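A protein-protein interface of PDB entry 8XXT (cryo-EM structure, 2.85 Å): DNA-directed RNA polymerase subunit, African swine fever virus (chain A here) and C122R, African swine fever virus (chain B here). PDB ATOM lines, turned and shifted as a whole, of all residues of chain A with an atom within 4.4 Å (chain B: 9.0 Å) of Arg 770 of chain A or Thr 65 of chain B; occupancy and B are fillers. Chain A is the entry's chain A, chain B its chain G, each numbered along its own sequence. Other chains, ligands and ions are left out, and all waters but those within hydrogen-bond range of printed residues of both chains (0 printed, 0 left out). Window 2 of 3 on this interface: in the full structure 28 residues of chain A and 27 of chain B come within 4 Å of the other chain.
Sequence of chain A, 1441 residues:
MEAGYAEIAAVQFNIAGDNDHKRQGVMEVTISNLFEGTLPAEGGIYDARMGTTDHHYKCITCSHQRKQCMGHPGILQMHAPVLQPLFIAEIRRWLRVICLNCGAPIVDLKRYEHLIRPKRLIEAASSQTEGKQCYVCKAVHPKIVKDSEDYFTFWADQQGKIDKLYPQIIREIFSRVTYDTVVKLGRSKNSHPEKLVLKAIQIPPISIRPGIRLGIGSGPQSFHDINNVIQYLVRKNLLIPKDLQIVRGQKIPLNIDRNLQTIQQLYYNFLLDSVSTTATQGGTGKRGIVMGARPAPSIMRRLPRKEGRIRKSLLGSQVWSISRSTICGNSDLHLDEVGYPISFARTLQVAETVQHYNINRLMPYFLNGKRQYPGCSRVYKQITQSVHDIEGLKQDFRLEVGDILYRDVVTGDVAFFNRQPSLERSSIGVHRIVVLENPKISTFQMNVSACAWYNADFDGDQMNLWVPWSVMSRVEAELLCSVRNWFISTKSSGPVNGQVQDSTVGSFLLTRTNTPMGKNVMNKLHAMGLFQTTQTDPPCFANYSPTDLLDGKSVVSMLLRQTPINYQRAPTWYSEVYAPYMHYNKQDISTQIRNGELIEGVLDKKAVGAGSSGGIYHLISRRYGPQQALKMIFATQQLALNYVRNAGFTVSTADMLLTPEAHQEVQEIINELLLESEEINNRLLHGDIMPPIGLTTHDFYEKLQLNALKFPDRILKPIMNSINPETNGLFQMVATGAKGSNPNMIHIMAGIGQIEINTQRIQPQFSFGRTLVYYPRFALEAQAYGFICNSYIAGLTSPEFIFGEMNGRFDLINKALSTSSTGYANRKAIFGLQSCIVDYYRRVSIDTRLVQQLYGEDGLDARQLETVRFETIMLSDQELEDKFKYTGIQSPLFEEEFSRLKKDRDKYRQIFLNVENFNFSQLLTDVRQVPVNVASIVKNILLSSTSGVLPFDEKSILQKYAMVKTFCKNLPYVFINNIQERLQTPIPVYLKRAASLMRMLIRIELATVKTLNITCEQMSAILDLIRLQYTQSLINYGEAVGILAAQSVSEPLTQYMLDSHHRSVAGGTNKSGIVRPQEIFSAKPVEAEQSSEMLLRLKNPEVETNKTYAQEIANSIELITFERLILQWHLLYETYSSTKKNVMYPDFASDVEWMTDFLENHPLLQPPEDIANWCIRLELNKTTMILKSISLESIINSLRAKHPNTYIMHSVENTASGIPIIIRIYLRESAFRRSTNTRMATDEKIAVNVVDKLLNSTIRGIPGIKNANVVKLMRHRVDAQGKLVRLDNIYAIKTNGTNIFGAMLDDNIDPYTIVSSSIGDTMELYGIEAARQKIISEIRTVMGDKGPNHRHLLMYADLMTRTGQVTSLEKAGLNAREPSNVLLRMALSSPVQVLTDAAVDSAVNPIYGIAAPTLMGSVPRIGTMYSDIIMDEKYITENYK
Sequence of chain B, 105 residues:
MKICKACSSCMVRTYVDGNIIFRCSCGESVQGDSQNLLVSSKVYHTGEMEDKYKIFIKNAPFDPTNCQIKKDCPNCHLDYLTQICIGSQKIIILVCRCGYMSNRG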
ATOM      1  N   PRO A 764      15.512 -15.441  22.964  1.00  0.00           N
ATOM      2  CA  PRO A 764      14.463 -15.380  23.989  1.00  0.00           C
ATOM      3  C   PRO A 764      14.771 -16.252  25.194  1.00  0.00           C
ATOM      4  O   PRO A 764      14.305 -17.392  25.278  1.00  0.00           O
ATOM      5  CB  PRO A 764      13.220 -15.872  23.242  1.00  0.00           C
ATOM      6  CG  PRO A 764      13.748 -16.707  22.145  1.00  0.00           C
ATOM      7  CD  PRO A 764      15.042 -16.085  21.729  1.00  0.00           C
ATOM      8  N   GLN A 765      15.556 -15.725  26.134  1.00  0.00           N
ATOM      9  CA  GLN A 765      15.981 -16.487  27.299  1.00  0.00           C
ATOM     10  C   GLN A 765      15.172 -16.197  28.554  1.00  0.00           C
ATOM     11  O   GLN A 765      15.240 -16.980  29.504  1.00  0.00           O
ATOM     12  CB  GLN A 765      17.461 -16.223  27.598  1.00  0.00           C
ATOM     13  CG  GLN A 765      18.375 -16.397  26.401  1.00  0.00           C
ATOM     14  CD  GLN A 765      18.700 -17.848  26.117  1.00  0.00           C
ATOM     15  OE1 GLN A 765      18.146 -18.755  26.737  1.00  0.00           O
ATOM     16  NE2 GLN A 765      19.597 -18.074  25.168  1.00  0.00           N
ATOM     17  N   PHE A 766      14.425 -15.093  28.590  1.00  0.00           N
ATOM     18  CA  PHE A 766      13.663 -14.768  29.790  1.00  0.00           C
ATOM     19  C   PHE A 766      12.606 -15.823  30.074  1.00  0.00           C
ATOM     20  O   PHE A 766      12.400 -16.218  31.226  1.00  0.00           O
ATOM     21  CB  PHE A 766      13.011 -13.397  29.646  1.00  0.00           C
ATOM     22  CG  PHE A 766      12.201 -12.987  30.835  1.00  0.00           C
ATOM     23  CD1 PHE A 766      12.805 -12.779  32.057  1.00  0.00           C
ATOM     24  CD2 PHE A 766      10.837 -12.815  30.734  1.00  0.00           C
ATOM     25  CE1 PHE A 766      12.062 -12.403  33.152  1.00  0.00           C
ATOM     26  CE2 PHE A 766      10.093 -12.441  31.826  1.00  0.00           C
ATOM     27  CZ  PHE A 766      10.706 -12.235  33.036  1.00  0.00           C
ATOM     28  N   SER A 767      11.929 -16.289  29.033  1.00  0.00           N
ATOM     29  CA  SER A 767      10.860 -17.266  29.153  1.00  0.00           C
ATOM     30  C   SER A 767      10.688 -17.918  27.788  1.00  0.00           C
ATOM     31  O   SER A 767      11.502 -17.717  26.881  1.00  0.00           O
ATOM     32  CB  SER A 767       9.572 -16.602  29.654  1.00  0.00           C
ATOM     33  OG  SER A 767       8.531 -17.547  29.806  1.00  0.00           O
ATOM     34  N   PHE A 768       9.632 -18.705  27.636  1.00  0.00           N
ATOM     35  CA  PHE A 768       9.328 -19.291  26.338  1.00  0.00           C
ATOM     36  C   PHE A 768       8.819 -18.199  25.411  1.00  0.00           C
ATOM     37  O   PHE A 768       7.682 -17.746  25.549  1.00  0.00           O
ATOM     38  CB  PHE A 768       8.297 -20.404  26.477  1.00  0.00           C
ATOM     39  CG  PHE A 768       7.684 -20.817  25.172  1.00  0.00           C
ATOM     40  CD1 PHE A 768       8.481 -21.230  24.121  1.00  0.00           C
ATOM     41  CD2 PHE A 768       6.317 -20.777  24.992  1.00  0.00           C
ATOM     42  CE1 PHE A 768       7.922 -21.600  22.921  1.00  0.00           C
ATOM     43  CE2 PHE A 768       5.757 -21.149  23.792  1.00  0.00           C
ATOM     44  CZ  PHE A 768       6.560 -21.558  22.756  1.00  0.00           C
ATOM     45  N   GLY A 769       9.650 -17.775  24.464  1.00  0.00           N
ATOM     46  CA  GLY A 769       9.251 -16.760  23.512  1.00  0.00           C
ATOM     47  C   GLY A 769       9.441 -15.333  23.966  1.00  0.00           C
ATOM     48  O   GLY A 769       9.080 -14.415  23.223  1.00  0.00           O
ATOM     49  N   ARG A 770       9.998 -15.110  25.150  1.00  0.00           N
ATOM     50  CA  ARG A 770      10.230 -13.772  25.668  1.00  0.00           C
ATOM     51  C   ARG A 770      11.723 -13.501  25.756  1.00  0.00           C
ATOM     52  O   ARG A 770      12.489 -14.347  26.222  1.00  0.00           O
ATOM     53  CB  ARG A 770       9.607 -13.595  27.053  1.00  0.00           C
ATOM     54  CG  ARG A 770       8.123 -13.825  27.103  1.00  0.00           C
ATOM     55  CD  ARG A 770       7.564 -13.412  28.443  1.00  0.00           C
ATOM     56  NE  ARG A 770       7.513 -11.965  28.582  1.00  0.00           N
ATOM     57  CZ  ARG A 770       7.109 -11.335  29.675  1.00  0.00           C
ATOM     58  NH1 ARG A 770       6.717 -11.998  30.747  1.00  0.00           N
ATOM     59  NH2 ARG A 770       7.102 -10.009  29.692  1.00  0.00           N
ATOM     60  N   THR A 771      12.130 -12.316  25.311  1.00  0.00           N
ATOM     61  CA  THR A 771      13.510 -11.888  25.475  1.00  0.00           C
ATOM     62  C   THR A 771      13.729 -11.122  26.769  1.00  0.00           C
ATOM     63  O   THR A 771      14.822 -11.185  27.337  1.00  0.00           O
ATOM     64  CB  THR A 771      13.942 -11.020  24.292  1.00  0.00           C
ATOM     65  OG1 THR A 771      13.089  -9.876  24.204  1.00  0.00           O
ATOM     66  CG2 THR A 771      13.841 -11.803  23.004  1.00  0.00           C
ATOM     67  N   LEU A 772      12.712 -10.410  27.248  1.00  0.00           N
ATOM     68  CA  LEU A 772      12.805  -9.648  28.485  1.00  0.00           C
ATOM     69  C   LEU A 772      11.413  -9.487  29.070  1.00  0.00           C
ATOM     70  O   LEU A 772      10.406  -9.700  28.394  1.00  0.00           O
ATOM     71  CB  LEU A 772      13.436  -8.270  28.265  1.00  0.00           C
ATOM     72  CG  LEU A 772      14.953  -8.140  28.327  1.00  0.00           C
ATOM     73  CD1 LEU A 772      15.357  -6.712  28.048  1.00  0.00           C
ATOM     74  CD2 LEU A 772      15.452  -8.576  29.683  1.00  0.00           C
ATOM     75  N   VAL A 773      11.369  -9.098  30.345  1.00  0.00           N
ATOM     76  CA  VAL A 773      10.093  -8.833  30.997  1.00  0.00           C
ATOM     77  C   VAL A 773       9.428  -7.589  30.430  1.00  0.00           C
ATOM     78  O   VAL A 773       8.231  -7.375  30.640  1.00  0.00           O
ATOM     79  CB  VAL A 773      10.294  -8.710  32.519  1.00  0.00           C
ATOM     80  CG1 VAL A 773      10.958  -7.396  32.863  1.00  0.00           C
ATOM     81  CG2 VAL A 773       8.974  -8.858  33.252  1.00  0.00           C
ATOM     82  N   TYR A 775       9.043  -6.967  27.238  1.00  0.00           N
ATOM     83  CA  TYR A 775       8.500  -7.242  25.922  1.00  0.00           C
ATOM     84  C   TYR A 775       7.533  -8.411  25.991  1.00  0.00           C
ATOM     85  O   TYR A 775       7.711  -9.325  26.800  1.00  0.00           O
ATOM     86  CB  TYR A 775       9.623  -7.551  24.924  1.00  0.00           C
ATOM     87  CG  TYR A 775      10.555  -6.385  24.736  1.00  0.00           C
ATOM     88  CD1 TYR A 775      10.148  -5.255  24.049  1.00  0.00           C
ATOM     89  CD2 TYR A 775      11.831  -6.401  25.272  1.00  0.00           C
ATOM     90  CE1 TYR A 775      10.987  -4.182  23.887  1.00  0.00           C
ATOM     91  CE2 TYR A 775      12.679  -5.331  25.116  1.00  0.00           C
ATOM     92  CZ  TYR A 775      12.251  -4.223  24.423  1.00  0.00           C
ATOM     93  OH  TYR A 775      13.093  -3.151  24.262  1.00  0.00           O
ATOM     94  N   PRO A 776       6.497  -8.402  25.160  1.00  0.00           N
ATOM     95  CA  PRO A 776       5.514  -9.483  25.197  1.00  0.00           C
ATOM     96  C   PRO A 776       6.052 -10.753  24.563  1.00  0.00           C
ATOM     97  O   PRO A 776       7.027 -10.748  23.811  1.00  0.00           O
ATOM     98  CB  PRO A 776       4.341  -8.919  24.397  1.00  0.00           C
ATOM     99  CG  PRO A 776       4.969  -7.965  23.461  1.00  0.00           C
ATOM    100  CD  PRO A 776       6.133  -7.361  24.187  1.00  0.00           C
ATOM    101  N   ARG A 777       5.393 -11.857  24.886  1.00  0.00           N
ATOM    102  CA  ARG A 777       5.768 -13.143  24.323  1.00  0.00           C
ATOM    103  C   ARG A 777       5.521 -13.154  22.821  1.00  0.00           C
ATOM    104  O   ARG A 777       4.462 -12.730  22.353  1.00  0.00           O
ATOM    105  CB  ARG A 777       4.970 -14.251  25.001  1.00  0.00           C
ATOM    106  CG  ARG A 777       5.639 -15.596  24.982  1.00  0.00           C
ATOM    107  CD  ARG A 777       4.731 -16.657  25.560  1.00  0.00           C
ATOM    108  NE  ARG A 777       4.126 -16.233  26.814  1.00  0.00           N
ATOM    109  CZ  ARG A 777       4.654 -16.448  28.009  1.00  0.00           C
ATOM    110  NH1 ARG A 777       5.806 -17.079  28.150  1.00  0.00           N
ATOM    111  NH2 ARG A 777       4.010 -16.021  29.089  1.00  0.00           N
ATOM    112  N   PHE B  56      -0.745 -24.577  26.223  1.00  0.00           N
ATOM    113  CA  PHE B  56      -0.276 -23.209  26.048  1.00  0.00           C
ATOM    114  C   PHE B  56      -1.208 -22.421  25.140  1.00  0.00           C
ATOM    115  O   PHE B  56      -1.527 -21.265  25.427  1.00  0.00           O
ATOM    116  CB  PHE B  56       1.144 -23.206  25.491  1.00  0.00           C
ATOM    117  CG  PHE B  56       1.665 -21.837  25.194  1.00  0.00           C
ATOM    118  CD1 PHE B  56       2.211 -21.064  26.199  1.00  0.00           C
ATOM    119  CD2 PHE B  56       1.604 -21.319  23.915  1.00  0.00           C
ATOM    120  CE1 PHE B  56       2.687 -19.804  25.935  1.00  0.00           C
ATOM    121  CE2 PHE B  56       2.078 -20.059  23.648  1.00  0.00           C
ATOM    122  CZ  PHE B  56       2.621 -19.301  24.658  1.00  0.00           C
ATOM    123  N   ASN B  59      -4.426 -21.576  27.017  1.00  0.00           N
ATOM    124  CA  ASN B  59      -4.280 -20.537  28.027  1.00  0.00           C
ATOM    125  C   ASN B  59      -3.773 -19.216  27.468  1.00  0.00           C
ATOM    126  O   ASN B  59      -3.781 -18.218  28.192  1.00  0.00           O
ATOM    127  CB  ASN B  59      -3.335 -21.013  29.125  1.00  0.00           C
ATOM    128  CG  ASN B  59      -4.016 -21.919  30.117  1.00  0.00           C
ATOM    129  OD1 ASN B  59      -3.395 -22.809  30.692  1.00  0.00           O
ATOM    130  ND2 ASN B  59      -5.303 -21.698  30.326  1.00  0.00           N
ATOM    131  N   ALA B  60      -3.342 -19.183  26.211  1.00  0.00           N
ATOM    132  CA  ALA B  60      -2.746 -17.973  25.653  1.00  0.00           C
ATOM    133  C   ALA B  60      -3.631 -16.736  25.698  1.00  0.00           C
ATOM    134  O   ALA B  60      -3.113 -15.664  26.053  1.00  0.00           O
ATOM    135  CB  ALA B  60      -2.298 -18.251  24.215  1.00  0.00           C
ATOM    136  N   PRO B  61      -4.922 -16.780  25.354  1.00  0.00           N
ATOM    137  CA  PRO B  61      -5.729 -15.555  25.459  1.00  0.00           C
ATOM    138  C   PRO B  61      -5.806 -15.010  26.868  1.00  0.00           C
ATOM    139  O   PRO B  61      -6.112 -13.825  27.045  1.00  0.00           O
ATOM    140  CB  PRO B  61      -7.108 -15.996  24.954  1.00  0.00           C
ATOM    141  CG  PRO B  61      -6.846 -17.197  24.139  1.00  0.00           C
ATOM    142  CD  PRO B  61      -5.710 -17.892  24.800  1.00  0.00           C
ATOM    143  N   PHE B  62      -5.548 -15.837  27.876  1.00  0.00           N
ATOM    144  CA  PHE B  62      -5.582 -15.414  29.263  1.00  0.00           C
ATOM    145  C   PHE B  62      -4.212 -15.040  29.808  1.00  0.00           C
ATOM    146  O   PHE B  62      -4.124 -14.576  30.948  1.00  0.00           O
ATOM    147  CB  PHE B  62      -6.197 -16.525  30.119  1.00  0.00           C
ATOM    148  CG  PHE B  62      -7.455 -17.094  29.536  1.00  0.00           C
ATOM    149  CD1 PHE B  62      -8.665 -16.457  29.722  1.00  0.00           C
ATOM    150  CD2 PHE B  62      -7.421 -18.249  28.777  1.00  0.00           C
ATOM    151  CE1 PHE B  62      -9.818 -16.970  29.178  1.00  0.00           C
ATOM    152  CE2 PHE B  62      -8.572 -18.766  28.229  1.00  0.00           C
ATOM    153  CZ  PHE B  62      -9.772 -18.126  28.429  1.00  0.00           C
ATOM    154  N   ASP B  63      -3.154 -15.225  29.031  1.00  0.00           N
ATOM    155  CA  ASP B  63      -1.817 -14.863  29.482  1.00  0.00           C
ATOM    156  C   ASP B  63      -1.603 -13.368  29.293  1.00  0.00           C
ATOM    157  O   ASP B  63      -1.710 -12.876  28.165  1.00  0.00           O
ATOM    158  CB  ASP B  63      -0.763 -15.642  28.711  1.00  0.00           C
ATOM    159  CG  ASP B  63       0.566 -15.699  29.435  1.00  0.00           C
ATOM    160  OD1 ASP B  63       0.647 -15.202  30.575  1.00  0.00           O
ATOM    161  OD2 ASP B  63       1.533 -16.241  28.864  1.00  0.00           O
ATOM    162  N   PRO B  64      -1.319 -12.611  30.354  1.00  0.00           N
ATOM    163  CA  PRO B  64      -1.067 -11.175  30.177  1.00  0.00           C
ATOM    164  C   PRO B  64       0.139 -10.876  29.310  1.00  0.00           C
ATOM    165  O   PRO B  64       0.160  -9.849  28.622  1.00  0.00           O
ATOM    166  CB  PRO B  64      -0.858 -10.677  31.613  1.00  0.00           C
ATOM    167  CG  PRO B  64      -1.492 -11.706  32.476  1.00  0.00           C
ATOM    168  CD  PRO B  64      -1.301 -13.006  31.770  1.00  0.00           C
ATOM    169  N   THR B  65       1.140 -11.747  29.314  1.00  0.00           N
ATOM    170  CA  THR B  65       2.417 -11.479  28.672  1.00  0.00           C
ATOM    171  C   THR B  65       2.448 -11.868  27.201  1.00  0.00           C
ATOM    172  O   THR B  65       3.478 -11.670  26.549  1.00  0.00           O
ATOM    173  CB  THR B  65       3.529 -12.213  29.417  1.00  0.00           C
ATOM    174  OG1 THR B  65       3.421 -13.619  29.170  1.00  0.00           O
ATOM    175  CG2 THR B  65       3.401 -11.970  30.901  1.00  0.00           C
ATOM    176  N   ASN B  66       1.366 -12.418  26.661  1.00  0.00           N
ATOM    177  CA  ASN B  66       1.343 -12.760  25.249  1.00  0.00           C
ATOM    178  C   ASN B  66       1.128 -11.512  24.401  1.00  0.00           C
ATOM    179  O   ASN B  66       0.386 -10.602  24.773  1.00  0.00           O
ATOM    180  CB  ASN B  66       0.247 -13.783  24.962  1.00  0.00           C
ATOM    181  CG  ASN B  66       0.778 -15.196  24.896  1.00  0.00           C
ATOM    182  OD1 ASN B  66       0.475 -16.026  25.749  1.00  0.00           O
ATOM    183  ND2 ASN B  66       1.573 -15.478  23.876  1.00  0.00           N
ATOM    184  N   CYS B  67       1.802 -11.472  23.254  1.00  0.00           N
ATOM    185  CA  CYS B  67       1.666 -10.351  22.339  1.00  0.00           C
ATOM    186  C   CYS B  67       0.291 -10.370  21.692  1.00  0.00           C
ATOM    187  O   CYS B  67      -0.270 -11.434  21.421  1.00  0.00           O
ATOM    188  CB  CYS B  67       2.751 -10.397  21.266  1.00  0.00           C
ATOM    189  SG  CYS B  67       2.659  -9.074  20.045  1.00  0.00           S
ATOM    190  N   GLN B  68      -0.253  -9.183  21.449  1.00  0.00           N
ATOM    191  CA  GLN B  68      -1.586  -9.038  20.888  1.00  0.00           C
ATOM    192  C   GLN B  68      -1.541  -8.092  19.700  1.00  0.00           C
ATOM    193  O   GLN B  68      -0.668  -7.227  19.606  1.00  0.00           O
ATOM    194  CB  GLN B  68      -2.573  -8.531  21.938  1.00  0.00           C
ATOM    195  CG  GLN B  68      -2.506  -9.321  23.221  1.00  0.00           C
ATOM    196  CD  GLN B  68      -3.662  -9.048  24.138  1.00  0.00           C
ATOM    197  OE1 GLN B  68      -4.671  -8.481  23.732  1.00  0.00           O
ATOM    198  NE2 GLN B  68      -3.529  -9.465  25.388  1.00  0.00           N
ATOM    199  N   THR B  82      -4.984 -12.375  20.181  1.00  0.00           N
ATOM    200  CA  THR B  82      -3.717 -12.803  20.758  1.00  0.00           C
ATOM    201  C   THR B  82      -2.913 -13.531  19.690  1.00  0.00           C
ATOM    202  O   THR B  82      -3.371 -14.538  19.143  1.00  0.00           O
ATOM    203  CB  THR B  82      -3.939 -13.702  21.970  1.00  0.00           C
ATOM    204  OG1 THR B  82      -4.800 -13.040  22.902  1.00  0.00           O
ATOM    205  CG2 THR B  82      -2.618 -14.007  22.645  1.00  0.00           C
ATOM    206  N   GLN B  83      -1.718 -13.026  19.403  1.00  0.00           N
ATOM    207  CA  GLN B  83      -0.878 -13.547  18.334  1.00  0.00           C
ATOM    208  C   GLN B  83       0.149 -14.507  18.912  1.00  0.00           C
ATOM    209  O   GLN B  83       0.778 -14.213  19.933  1.00  0.00           O
ATOM    210  CB  GLN B  83      -0.181 -12.413  17.588  1.00  0.00           C
ATOM    211  CG  GLN B  83       0.710 -12.871  16.462  1.00  0.00           C
ATOM    212  CD  GLN B  83       1.778 -11.856  16.142  1.00  0.00           C
ATOM    213  OE1 GLN B  83       1.791 -11.268  15.061  1.00  0.00           O
ATOM    214  NE2 GLN B  83       2.699 -11.659  17.073  1.00  0.00           N
ATOM    215  N   CYS B  85       3.299 -17.436  18.013  1.00  0.00           N
ATOM    216  CA  CYS B  85       4.291 -17.950  17.075  1.00  0.00           C
ATOM    217  C   CYS B  85       4.961 -19.176  17.678  1.00  0.00           C
ATOM    218  O   CYS B  85       5.632 -19.076  18.710  1.00  0.00           O
ATOM    219  CB  CYS B  85       5.327 -16.879  16.737  1.00  0.00           C
ATOM    220  SG  CYS B  85       6.401 -17.280  15.353  1.00  0.00           S
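The backbone carbonyl oxygen of Phe 768 of chain A lies close to the guanidinium group of Arg 777 of chain A, 3.3 Å away.
NH2 of Arg 770 of chain A sits at hydrogen-bond distance from O of Tyr 775 of chain A (3.0 Å).
The side-chain hydroxyl of Ser 767 of chain A is in hydrogen-bond range of the guanidinium group of Arg 777 of chain A (3.2 Å).
OG1 of Thr 65 of chain B is in hydrogen-bond range of OD2 of Asp 63 of chain B, 3.2 Å away.
The backbone NH (N) of Gln 765 of chain A lies within hydrogen-bond range of the backbone carbonyl oxygen (O) of Arg 770 of chain A (3.4 Å).
The side-chain carboxylate (OD2) of Asp 63 of chain B sits close to the side-chain amide oxygen (OD1) of Asn 66 of chain B, 3.3 Å away.
Among the printed residues, pairs that only touch across the chains: Phe 768 of chain A with Phe 56 of chain B, Arg 770 of chain A with Thr 65 of chain B, Pro 776 of chain A with Thr 65 of chain B, Pro 776 of chain A with Cys 67 of chain B, Arg 777 of chain A with Phe 56 of chain B and Arg 777 of chain A with Asn 66 of chain B.
Of chain B, only Thr 65 (3.3 Å) comes within 4 Å of Arg 770 of chain A.
Of chain A, only Arg 770 (3.3 Å), Pro 776 (3.3 Å) and Arg 777 (2.5 Å) come within 4 Å of Thr 65 of chain B.
Ser 767 of chain A touches none of the printed residues of chain B.
No residue of chain B comes within 4 Å of Gly 769 of chain A.
No residue of chain B comes within 4 Å of Thr 771 of chain A.
Of chain B, only Phe 56 (3.5 Å), Asp 63 (2.5 Å), Thr 65 (2.5 Å), Asn 66 (3.8 Å) and Cys 67 (3.1 Å) come within 4 Å of Arg 777 of chain A.
Printed residues of chain A within 4 Å of Asn 66 of chain B: Arg 777.
Printed residues of chain B within 4 Å of Pro 776 of chain A: Thr 65 and Cys 67.
Pro 64 of chain B touches none of the printed residues of chain A.
Leu 772 of chain A touches none of the printed residues of chain B.
The nearest residue of chain B that does not touch Arg 770 of chain A is Asn 66 of chain B (6.5 Å).
The nearest printed residue of chain A that does not touch Asp 63 of chain B is Arg 770 of chain A (6.7 Å).
Printed residues of chain A that touch a printed residue of chain B: Phe 768, Arg 770, Pro 776 and Arg 777.
Hydrophobic or aromatic side chains of chain A that line the printed part of chain B: Phe 768 and Pro 776.
Printed residues of chain B that touch a printed residue of chain A: Phe 56, Asp 63, Thr 65, Asn 66 and Cys 67.
Hydrophobic or aromatic side chains of chain B that line the printed part of chain A: Phe 56.
Among the printed residues, Asp or Glu carboxylates within 4 Å of a Lys or Arg side-chain nitrogen of the other chain: Arg 777 of chain A with Asp 63 of chain B (2.5 Å).
The guanidinium group (NH2) of Arg 777 of chain A sits at hydrogen-bond distance from the side-chain hydroxyl (OG1) of Thr 65 of chain B.
The side-chain carboxylate (OD2) of Asp 63 of chain B is in salt-bridge range of the guanidinium group (NH2) of Arg 777 of chain A, 2.5 Å away.
O of Arg 777 of chain A sits at hydrogen-bond distance from N of Cys 67 of chain B, 3.1 Å away.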
